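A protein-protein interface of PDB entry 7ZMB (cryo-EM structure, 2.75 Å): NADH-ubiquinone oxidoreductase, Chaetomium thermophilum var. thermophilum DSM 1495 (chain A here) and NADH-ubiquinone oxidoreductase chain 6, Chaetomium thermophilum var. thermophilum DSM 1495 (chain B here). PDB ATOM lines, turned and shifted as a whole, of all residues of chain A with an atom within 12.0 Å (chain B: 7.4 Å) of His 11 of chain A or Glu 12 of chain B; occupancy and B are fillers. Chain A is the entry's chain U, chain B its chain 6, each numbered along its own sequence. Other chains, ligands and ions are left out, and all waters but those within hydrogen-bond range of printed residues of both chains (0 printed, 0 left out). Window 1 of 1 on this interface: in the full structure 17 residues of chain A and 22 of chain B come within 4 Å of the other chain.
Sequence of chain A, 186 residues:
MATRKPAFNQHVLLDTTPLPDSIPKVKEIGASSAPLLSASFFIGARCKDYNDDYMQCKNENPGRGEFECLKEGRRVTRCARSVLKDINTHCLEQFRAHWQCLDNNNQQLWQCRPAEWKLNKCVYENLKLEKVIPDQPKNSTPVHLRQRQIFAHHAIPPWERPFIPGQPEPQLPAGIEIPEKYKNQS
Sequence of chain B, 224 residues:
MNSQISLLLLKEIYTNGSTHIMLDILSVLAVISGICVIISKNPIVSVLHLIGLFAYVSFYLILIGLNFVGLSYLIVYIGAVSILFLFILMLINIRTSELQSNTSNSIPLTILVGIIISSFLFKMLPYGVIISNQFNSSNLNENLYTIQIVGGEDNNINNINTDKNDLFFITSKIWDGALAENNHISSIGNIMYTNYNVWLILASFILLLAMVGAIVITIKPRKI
The backbone NH (N) of Ala 2 of chain A is in hydrogen-bond range of the backbone carbonyl oxygen (O) of Ile 170 of chain B (3.2 Å).
The backbone carbonyl oxygen (O) of Leu 8 of chain B lies close to the backbone carbonyl oxygen (O) of Val 12 of chain A (3.3 Å).
ND2 of Asn 16 of chain B sits at hydrogen-bond distance from OE1 of Gln 10 of chain A (3.2 Å).
The side-chain amide oxygen of Gln 10 of chain A lies close to the backbone carbonyl oxygen of Gly 17 of chain B, 2.9 Å away.
N of Gly 17 of chain B is in hydrogen-bond range of O of Asn 9 of chain A, at 2.8 Å.
The backbone carbonyl oxygen of Leu 8 of chain B is in hydrogen-bond range of the backbone NH of Leu 14 of chain A, at 3.0 Å.
N of Val 12 of chain A lies within hydrogen-bond range of O of Leu 10 of chain B (2.7 Å).
ND2 of Asn 9 of chain A is in hydrogen-bond range of OE1 of Glu 12 of chain B.
The backbone carbonyl oxygen of Gln 10 of chain A lies within hydrogen-bond range of the backbone NH of Glu 12 of chain B, at 3.1 Å.
O of Thr 15 of chain B lies within hydrogen-bond range of ND2 of Asn 9 of chain A.
The side-chain amide oxygen (OD1) of Asn 16 of chain B sits close to the backbone carbonyl oxygen (O) of Tyr 14 of chain B (3.4 Å).
The side-chain hydroxyl (OG1) of Thr 15 of chain B is in hydrogen-bond range of the side-chain carboxylate (OE2) of Glu 12 of chain B, 3.1 Å away.
The backbone carbonyl oxygen of Ile 13 of chain B sits close to the side-chain amide oxygen of Asn 16 of chain B (3.1 Å).
Among the printed residues, pairs that only touch across the chains: Asn 9 of chain A with Asn 16 of chain B (3.1 Å), Leu 13 of chain A with Leu 8 of chain B (3.3 Å), His 11 of chain A with Leu 10 of chain B (3.3 Å), Ala 7 of chain A with Gly 17 of chain B (3.3 Å), Met 1 of chain A with Ile 170 of chain B (3.5 Å), His 11 of chain A with Leu 9 of chain B (3.5 Å), Arg 4 of chain A with Phe 169 of chain B (3.6 Å), Val 12 of chain A with Leu 9 of chain B (3.6 Å), Gln 10 of chain A with Lys 11 of chain B (3.7 Å), His 11 of chain A with Glu 12 of chain B (3.7 Å), His 11 of chain A with Lys 11 of chain B (3.9 Å), Val 12 of chain A with Glu 12 of chain B (3.9 Å) and Leu 13 of chain A with Ile 170 of chain B (3.98 Å).
Of the printed residues of chain B, Met 1 of chain A touches Ile 170 (3.5 Å).
Of the printed residues of chain B, Arg 4 of chain A touches Phe 169 (3.6 Å).
Lys 5 of chain A touches none of the printed residues of chain B.
Of the printed residues of chain B, Gln 10 of chain A touches Lys 11, Glu 12, Asn 16 and Gly 17.
His 11 of chain A touches four residues of chain B.
Of the printed residues of chain B, Leu 13 of chain A touches Leu 8 (3.3 Å) and Ile 170 (3.98 Å).
Leu 9 of chain B touches two residues of chain A.
Leu 10 of chain B touches just these residues of chain A: His 11 (3.3 Å) and Val 12 (2.7 Å).
Glu 12 of chain B touches just these residues of chain A: Asn 9 (2.8 Å), Gln 10 (3.1 Å), His 11 (3.7 Å) and Val 12 (3.9 Å).
No residue of chain A comes within 4 Å of Ile 13 of chain B.
Tyr 14 of chain B touches none of the printed residues of chain A.
Of the printed residues of chain A, Thr 15 of chain B touches Asn 9.
Of chain A, only Ala 7, Asn 9 and Gln 10 come within 4 Å of Gly 17 of chain B.
Of the 13 printed residues of chain B, 10 touch a printed residue of chain A.
Hydrophobic or aromatic side chains of chain B within 4 Å of the printed part of chain A: Leu 8, Leu 9, Leu 10, Phe 169 and Ile 170.
Among the printed residues, 23 pairs touch across the chains.
Among the printed residues, no Asp or Glu carboxylate lies within 4 Å of a Lys or Arg side-chain nitrogen of the other chain.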
ATOM      1  N   MET A   1      15.784  21.226   2.230  1.00  0.00           N
ATOM      2  CA  MET A   1      16.278  20.176   3.151  1.00  0.00           C
ATOM      3  C   MET A   1      15.115  19.294   3.595  1.00  0.00           C
ATOM      4  O   MET A   1      13.971  19.723   3.413  1.00  0.00           O
ATOM      5  CB  MET A   1      17.008  20.793   4.339  1.00  0.00           C
ATOM      6  N   ALA A   2      15.389  18.163   4.242  1.00  0.00           N
ATOM      7  CA  ALA A   2      14.345  17.164   4.560  1.00  0.00           C
ATOM      8  C   ALA A   2      13.270  17.674   5.521  1.00  0.00           C
ATOM      9  O   ALA A   2      13.540  18.605   6.296  1.00  0.00           O
ATOM     10  CB  ALA A   2      15.008  15.933   5.097  1.00  0.00           C
ATOM     11  N   ARG A   4      11.919  15.813   7.765  1.00  0.00           N
ATOM     12  CA  ARG A   4      12.024  15.024   9.009  1.00  0.00           C
ATOM     13  C   ARG A   4      12.326  15.991  10.143  1.00  0.00           C
ATOM     14  O   ARG A   4      13.058  16.960   9.918  1.00  0.00           O
ATOM     15  CB  ARG A   4      13.081  13.922   8.918  1.00  0.00           C
ATOM     16  CG  ARG A   4      14.502  14.412   8.711  1.00  0.00           C
ATOM     17  CD  ARG A   4      15.465  13.381   9.245  1.00  0.00           C
ATOM     18  NE  ARG A   4      16.832  13.873   9.304  1.00  0.00           N
ATOM     19  CZ  ARG A   4      17.410  14.351  10.397  1.00  0.00           C
ATOM     20  NH1 ARG A   4      18.664  14.765  10.358  1.00  0.00           N
ATOM     21  NH2 ARG A   4      16.733  14.416  11.528  1.00  0.00           N
ATOM     22  N   LYS A   5      11.718  15.751  11.306  1.00  0.00           N
ATOM     23  CA  LYS A   5      11.995  16.605  12.481  1.00  0.00           C
ATOM     24  C   LYS A   5      13.298  16.121  13.127  1.00  0.00           C
ATOM     25  O   LYS A   5      13.364  14.944  13.511  1.00  0.00           O
ATOM     26  CB  LYS A   5      10.805  16.518  13.431  1.00  0.00           C
ATOM     27  CG  LYS A   5       9.442  16.647  12.767  1.00  0.00           C
ATOM     28  CD  LYS A   5       8.297  16.294  13.691  1.00  0.00           C
ATOM     29  CE  LYS A   5       8.423  14.903  14.275  1.00  0.00           C
ATOM     30  NZ  LYS A   5       7.344  14.621  15.251  1.00  0.00           N
ATOM     31  N   PRO A   6      14.326  16.986  13.273  1.00  0.00           N
ATOM     32  CA  PRO A   6      15.633  16.582  13.816  1.00  0.00           C
ATOM     33  C   PRO A   6      15.682  16.175  15.296  1.00  0.00           C
ATOM     34  O   PRO A   6      14.952  16.742  16.085  1.00  0.00           O
ATOM     35  CB  PRO A   6      16.482  17.846  13.628  1.00  0.00           C
ATOM     36  CG  PRO A   6      15.487  18.979  13.615  1.00  0.00           C
ATOM     37  CD  PRO A   6      14.284  18.403  12.905  1.00  0.00           C
ATOM     38  N   ALA A   7      16.538  15.209  15.634  1.00  0.00           N
ATOM     39  CA  ALA A   7      16.693  14.775  17.041  1.00  0.00           C
ATOM     40  C   ALA A   7      18.107  15.067  17.553  1.00  0.00           C
ATOM     41  O   ALA A   7      18.275  15.129  18.783  1.00  0.00           O
ATOM     42  CB  ALA A   7      16.381  13.309  17.153  1.00  0.00           C
ATOM     43  N   PHE A   8      19.077  15.241  16.656  1.00  0.00           N
ATOM     44  CA  PHE A   8      20.486  15.443  17.084  1.00  0.00           C
ATOM     45  C   PHE A   8      21.092  16.659  16.371  1.00  0.00           C
ATOM     46  O   PHE A   8      22.253  16.594  15.949  1.00  0.00           O
ATOM     47  CB  PHE A   8      21.300  14.157  16.898  1.00  0.00           C
ATOM     48  CG  PHE A   8      20.830  12.998  17.741  1.00  0.00           C
ATOM     49  CD1 PHE A   8      21.178  12.896  19.076  1.00  0.00           C
ATOM     50  CD2 PHE A   8      20.022  12.013  17.207  1.00  0.00           C
ATOM     51  CE1 PHE A   8      20.740  11.832  19.846  1.00  0.00           C
ATOM     52  CE2 PHE A   8      19.579  10.950  17.977  1.00  0.00           C
ATOM     53  CZ  PHE A   8      19.941  10.860  19.298  1.00  0.00           C
ATOM     54  N   ASN A   9      20.325  17.740  16.256  1.00  0.00           N
ATOM     55  CA  ASN A   9      20.784  18.963  15.540  1.00  0.00           C
ATOM     56  C   ASN A   9      21.552  19.899  16.479  1.00  0.00           C
ATOM     57  O   ASN A   9      20.928  20.509  17.333  1.00  0.00           O
ATOM     58  CB  ASN A   9      19.606  19.718  14.918  1.00  0.00           C
ATOM     59  CG  ASN A   9      18.439  19.938  15.860  1.00  0.00           C
ATOM     60  OD1 ASN A   9      17.973  19.011  16.513  1.00  0.00           O
ATOM     61  ND2 ASN A   9      17.946  21.162  15.922  1.00  0.00           N
ATOM     62  N   GLN A  10      22.868  19.978  16.335  1.00  0.00           N
ATOM     63  CA  GLN A  10      23.677  20.888  17.186  1.00  0.00           C
ATOM     64  C   GLN A  10      24.180  22.064  16.348  1.00  0.00           C
ATOM     65  O   GLN A  10      24.862  22.930  16.909  1.00  0.00           O
ATOM     66  CB  GLN A  10      24.826  20.108  17.828  1.00  0.00           C
ATOM     67  CG  GLN A  10      24.421  18.772  18.440  1.00  0.00           C
ATOM     68  CD  GLN A  10      23.674  18.899  19.747  1.00  0.00           C
ATOM     69  OE1 GLN A  10      22.712  19.655  19.873  1.00  0.00           O
ATOM     70  NE2 GLN A  10      24.100  18.133  20.734  1.00  0.00           N
ATOM     71  N   HIS A  11      23.817  22.114  15.064  1.00  0.00           N
ATOM     72  CA  HIS A  11      24.362  23.157  14.156  1.00  0.00           C
ATOM     73  C   HIS A  11      23.302  23.674  13.196  1.00  0.00           C
ATOM     74  O   HIS A  11      22.302  22.969  12.993  1.00  0.00           O
ATOM     75  CB  HIS A  11      25.565  22.610  13.369  1.00  0.00           C
ATOM     76  CG  HIS A  11      26.716  22.232  14.234  1.00  0.00           C
ATOM     77  ND1 HIS A  11      27.493  23.175  14.870  1.00  0.00           N
ATOM     78  CD2 HIS A  11      27.212  21.026  14.585  1.00  0.00           C
ATOM     79  CE1 HIS A  11      28.430  22.569  15.570  1.00  0.00           C
ATOM     80  NE2 HIS A  11      28.279  21.249  15.410  1.00  0.00           N
ATOM     81  N   VAL A  12      23.527  24.859  12.633  1.00  0.00           N
ATOM     82  CA  VAL A  12      22.588  25.460  11.640  1.00  0.00           C
ATOM     83  C   VAL A  12      23.417  25.873  10.417  1.00  0.00           C
ATOM     84  O   VAL A  12      24.562  26.314  10.608  1.00  0.00           O
ATOM     85  CB  VAL A  12      21.833  26.648  12.266  1.00  0.00           C
ATOM     86  CG1 VAL A  12      21.272  27.603  11.225  1.00  0.00           C
ATOM     87  CG2 VAL A  12      20.732  26.191  13.209  1.00  0.00           C
ATOM     88  N   LEU A  13      22.873  25.705   9.209  1.00  0.00           N
ATOM     89  CA  LEU A  13      23.593  26.086   7.969  1.00  0.00           C
ATOM     90  C   LEU A  13      22.833  27.173   7.209  1.00  0.00           C
ATOM     91  O   LEU A  13      21.632  26.987   6.981  1.00  0.00           O
ATOM     92  CB  LEU A  13      23.789  24.842   7.101  1.00  0.00           C
ATOM     93  CG  LEU A  13      24.640  25.024   5.846  1.00  0.00           C
ATOM     94  CD1 LEU A  13      26.052  25.458   6.201  1.00  0.00           C
ATOM     95  CD2 LEU A  13      24.672  23.738   5.044  1.00  0.00           C
ATOM     96  N   LEU A  14      23.516  28.259   6.852  1.00  0.00           N
ATOM     97  CA  LEU A  14      22.911  29.364   6.123  1.00  0.00           C
ATOM     98  C   LEU A  14      23.471  29.443   4.707  1.00  0.00           C
ATOM     99  O   LEU A  14      24.380  28.706   4.325  1.00  0.00           O
ATOM    100  CB  LEU A  14      23.119  30.696   6.854  1.00  0.00           C
ATOM    101  CG  LEU A  14      22.204  30.989   8.050  1.00  0.00           C
ATOM    102  CD1 LEU A  14      22.692  30.306   9.297  1.00  0.00           C
ATOM    103  CD2 LEU A  14      22.056  32.461   8.289  1.00  0.00           C
ATOM    104  N   ASP A  15      22.906  30.353   3.921  1.00  0.00           N
ATOM    105  CA  ASP A  15      23.288  30.514   2.521  1.00  0.00           C
ATOM    106  C   ASP A  15      23.110  31.972   2.127  1.00  0.00           C
ATOM    107  O   ASP A  15      21.988  32.410   1.864  1.00  0.00           O
ATOM    108  CB  ASP A  15      22.456  29.609   1.616  1.00  0.00           C
ATOM    109  CG  ASP A  15      23.160  29.293   0.311  1.00  0.00           C
ATOM    110  OD1 ASP A  15      24.391  29.087   0.338  1.00  0.00           O
ATOM    111  OD2 ASP A  15      22.484  29.248  -0.734  1.00  0.00           O
ATOM    112  N   LEU B   8      27.445  29.366   5.945  1.00  0.00           N
ATOM    113  CA  LEU B   8      27.662  29.699   7.369  1.00  0.00           C
ATOM    114  C   LEU B   8      27.349  28.504   8.252  1.00  0.00           C
ATOM    115  O   LEU B   8      26.187  28.066   8.261  1.00  0.00           O
ATOM    116  CB  LEU B   8      26.755  30.881   7.709  1.00  0.00           C
ATOM    117  CG  LEU B   8      27.048  32.144   6.900  1.00  0.00           C
ATOM    118  CD1 LEU B   8      26.106  33.271   7.276  1.00  0.00           C
ATOM    119  CD2 LEU B   8      28.493  32.569   7.075  1.00  0.00           C
ATOM    120  N   LEU B   9      28.356  28.026   8.985  1.00  0.00           N
ATOM    121  CA  LEU B   9      28.088  26.950   9.958  1.00  0.00           C
ATOM    122  C   LEU B   9      27.983  27.662  11.301  1.00  0.00           C
ATOM    123  O   LEU B   9      28.914  28.355  11.682  1.00  0.00           O
ATOM    124  CB  LEU B   9      29.208  25.909   9.908  1.00  0.00           C
ATOM    125  CG  LEU B   9      28.803  24.465  10.199  1.00  0.00           C
ATOM    126  CD1 LEU B   9      29.964  23.524   9.930  1.00  0.00           C
ATOM    127  CD2 LEU B   9      28.323  24.304  11.633  1.00  0.00           C
ATOM    128  N   LEU B  10      26.845  27.523  11.960  1.00  0.00           N
ATOM    129  CA  LEU B  10      26.609  28.240  13.226  1.00  0.00           C
ATOM    130  C   LEU B  10      26.184  27.193  14.240  1.00  0.00           C
ATOM    131  O   LEU B  10      25.441  26.297  13.846  1.00  0.00           O
ATOM    132  CB  LEU B  10      25.435  29.182  12.944  1.00  0.00           C
ATOM    133  CG  LEU B  10      25.070  30.139  14.065  1.00  0.00           C
ATOM    134  CD1 LEU B  10      26.239  31.066  14.338  1.00  0.00           C
ATOM    135  CD2 LEU B  10      23.828  30.934  13.690  1.00  0.00           C
ATOM    136  N   LYS B  11      26.645  27.297  15.482  1.00  0.00           N
ATOM    137  CA  LYS B  11      26.137  26.381  16.540  1.00  0.00           C
ATOM    138  C   LYS B  11      24.720  26.809  16.917  1.00  0.00           C
ATOM    139  O   LYS B  11      24.498  28.025  17.064  1.00  0.00           O
ATOM    140  CB  LYS B  11      27.030  26.440  17.780  1.00  0.00           C
ATOM    141  CG  LYS B  11      26.610  25.538  18.934  1.00  0.00           C
ATOM    142  CD  LYS B  11      27.549  25.584  20.119  1.00  0.00           C
ATOM    143  CE  LYS B  11      28.946  25.119  19.776  1.00  0.00           C
ATOM    144  NZ  LYS B  11      29.833  25.136  20.962  1.00  0.00           N
ATOM    145  N   GLU B  12      23.817  25.845  17.100  1.00  0.00           N
ATOM    146  CA  GLU B  12      22.423  26.143  17.516  1.00  0.00           C
ATOM    147  C   GLU B  12      22.394  26.491  19.011  1.00  0.00           C
ATOM    148  O   GLU B  12      22.839  25.663  19.813  1.00  0.00           O
ATOM    149  CB  GLU B  12      21.571  24.914  17.231  1.00  0.00           C
ATOM    150  CG  GLU B  12      20.118  25.232  16.944  1.00  0.00           C
ATOM    151  CD  GLU B  12      19.355  24.044  16.390  1.00  0.00           C
ATOM    152  OE1 GLU B  12      20.010  23.083  15.949  1.00  0.00           O
ATOM    153  OE2 GLU B  12      18.115  24.077  16.415  1.00  0.00           O
ATOM    154  N   ILE B  13      21.873  27.668  19.356  1.00  0.00           N
ATOM    155  CA  ILE B  13      21.869  28.145  20.769  1.00  0.00           C
ATOM    156  C   ILE B  13      20.864  27.307  21.556  1.00  0.00           C
ATOM    157  O   ILE B  13      21.303  26.553  22.447  1.00  0.00           O
ATOM    158  CB  ILE B  13      21.677  29.677  20.843  1.00  0.00           C
ATOM    159  CG1 ILE B  13      21.825  30.209  22.271  1.00  0.00           C
ATOM    160  CG2 ILE B  13      20.411  30.160  20.153  1.00  0.00           C
ATOM    161  CD1 ILE B  13      21.881  31.718  22.366  1.00  0.00           C
ATOM    162  N   TYR B  14      19.573  27.476  21.276  1.00  0.00           N
ATOM    163  CA  TYR B  14      18.553  26.671  21.922  1.00  0.00           C
ATOM    164  C   TYR B  14      17.989  25.780  20.833  1.00  0.00           C
ATOM    165  O   TYR B  14      18.573  25.691  19.749  1.00  0.00           O
ATOM    166  CB  TYR B  14      17.457  27.520  22.561  1.00  0.00           C
ATOM    167  CG  TYR B  14      17.946  28.451  23.640  1.00  0.00           C
ATOM    168  CD1 TYR B  14      18.602  29.630  23.323  1.00  0.00           C
ATOM    169  CD2 TYR B  14      17.753  28.153  24.980  1.00  0.00           C
ATOM    170  CE1 TYR B  14      19.050  30.479  24.300  1.00  0.00           C
ATOM    171  CE2 TYR B  14      18.204  29.001  25.966  1.00  0.00           C
ATOM    172  CZ  TYR B  14      18.847  30.165  25.620  1.00  0.00           C
ATOM    173  OH  TYR B  14      19.295  31.015  26.601  1.00  0.00           O
ATOM    174  N   THR B  15      16.874  25.117  21.094  1.00  0.00           N
ATOM    175  CA  THR B  15      16.157  24.350  20.084  1.00  0.00           C
ATOM    176  C   THR B  15      17.031  23.282  19.434  1.00  0.00           C
ATOM    177  O   THR B  15      16.619  22.662  18.447  1.00  0.00           O
ATOM    178  CB  THR B  15      15.562  25.266  19.004  1.00  0.00           C
ATOM    179  OG1 THR B  15      16.607  25.970  18.326  1.00  0.00           O
ATOM    180  CG2 THR B  15      14.648  26.287  19.641  1.00  0.00           C
ATOM    181  N   ASN B  16      18.229  23.056  19.962  1.00  0.00           N
ATOM    182  CA  ASN B  16      19.134  22.046  19.456  1.00  0.00           C
ATOM    183  C   ASN B  16      18.774  20.682  20.037  1.00  0.00           C
ATOM    184  O   ASN B  16      18.167  20.568  21.102  1.00  0.00           O
ATOM    185  CB  ASN B  16      20.577  22.405  19.794  1.00  0.00           C
ATOM    186  CG  ASN B  16      20.785  22.635  21.264  1.00  0.00           C
ATOM    187  OD1 ASN B  16      20.430  23.681  21.799  1.00  0.00           O
ATOM    188  ND2 ASN B  16      21.381  21.659  21.931  1.00  0.00           N
ATOM    189  N   GLY B  17      19.162  19.641  19.317  1.00  0.00           N
ATOM    190  CA  GLY B  17      18.815  18.294  19.691  1.00  0.00           C
ATOM    191  C   GLY B  17      19.753  17.732  20.733  1.00  0.00           C
ATOM    192  O   GLY B  17      20.560  18.430  21.347  1.00  0.00           O
ATOM    193  N   PHE B 168      26.736  15.465   6.523  1.00  0.00           N
ATOM    194  CA  PHE B 168      25.829  16.056   7.534  1.00  0.00           C
ATOM    195  C   PHE B 168      24.420  16.050   6.951  1.00  0.00           C
ATOM    196  O   PHE B 168      24.221  16.547   5.827  1.00  0.00           O
ATOM    197  CB  PHE B 168      26.312  17.441   7.962  1.00  0.00           C
ATOM    198  CG  PHE B 168      27.621  17.443   8.711  1.00  0.00           C
ATOM    199  CD1 PHE B 168      27.659  17.208  10.077  1.00  0.00           C
ATOM    200  CD2 PHE B 168      28.818  17.674   8.053  1.00  0.00           C
ATOM    201  CE1 PHE B 168      28.860  17.206  10.766  1.00  0.00           C
ATOM    202  CE2 PHE B 168      30.020  17.673   8.742  1.00  0.00           C
ATOM    203  CZ  PHE B 168      30.038  17.440  10.097  1.00  0.00           C
ATOM    204  N   PHE B 169      23.491  15.433   7.677  1.00  0.00           N
ATOM    205  CA  PHE B 169      22.080  15.436   7.232  1.00  0.00           C
ATOM    206  C   PHE B 169      21.537  16.850   7.410  1.00  0.00           C
ATOM    207  O   PHE B 169      21.837  17.483   8.429  1.00  0.00           O
ATOM    208  CB  PHE B 169      21.281  14.368   7.982  1.00  0.00           C
ATOM    209  CG  PHE B 169      21.758  12.949   7.819  1.00  0.00           C
ATOM    210  CD1 PHE B 169      21.303  12.164   6.774  1.00  0.00           C
ATOM    211  CD2 PHE B 169      22.642  12.389   8.725  1.00  0.00           C
ATOM    212  CE1 PHE B 169      21.727  10.852   6.635  1.00  0.00           C
ATOM    213  CE2 PHE B 169      23.072  11.080   8.579  1.00  0.00           C
ATOM    214  CZ  PHE B 169      22.615  10.315   7.534  1.00  0.00           C
ATOM    215  N   ILE B 170      20.783  17.331   6.425  1.00  0.00           N
ATOM    216  CA  ILE B 170      20.222  18.709   6.487  1.00  0.00           C
ATOM    217  C   ILE B 170      18.697  18.614   6.559  1.00  0.00           C
ATOM    218  O   ILE B 170      18.114  17.832   5.795  1.00  0.00           O
ATOM    219  CB  ILE B 170      20.738  19.562   5.312  1.00  0.00           C
ATOM    220  CG1 ILE B 170      20.427  21.047   5.497  1.00  0.00           C
ATOM    221  CG2 ILE B 170      20.283  19.033   3.962  1.00  0.00           C
ATOM    222  CD1 ILE B 170      21.375  21.746   6.431  1.00  0.00           C
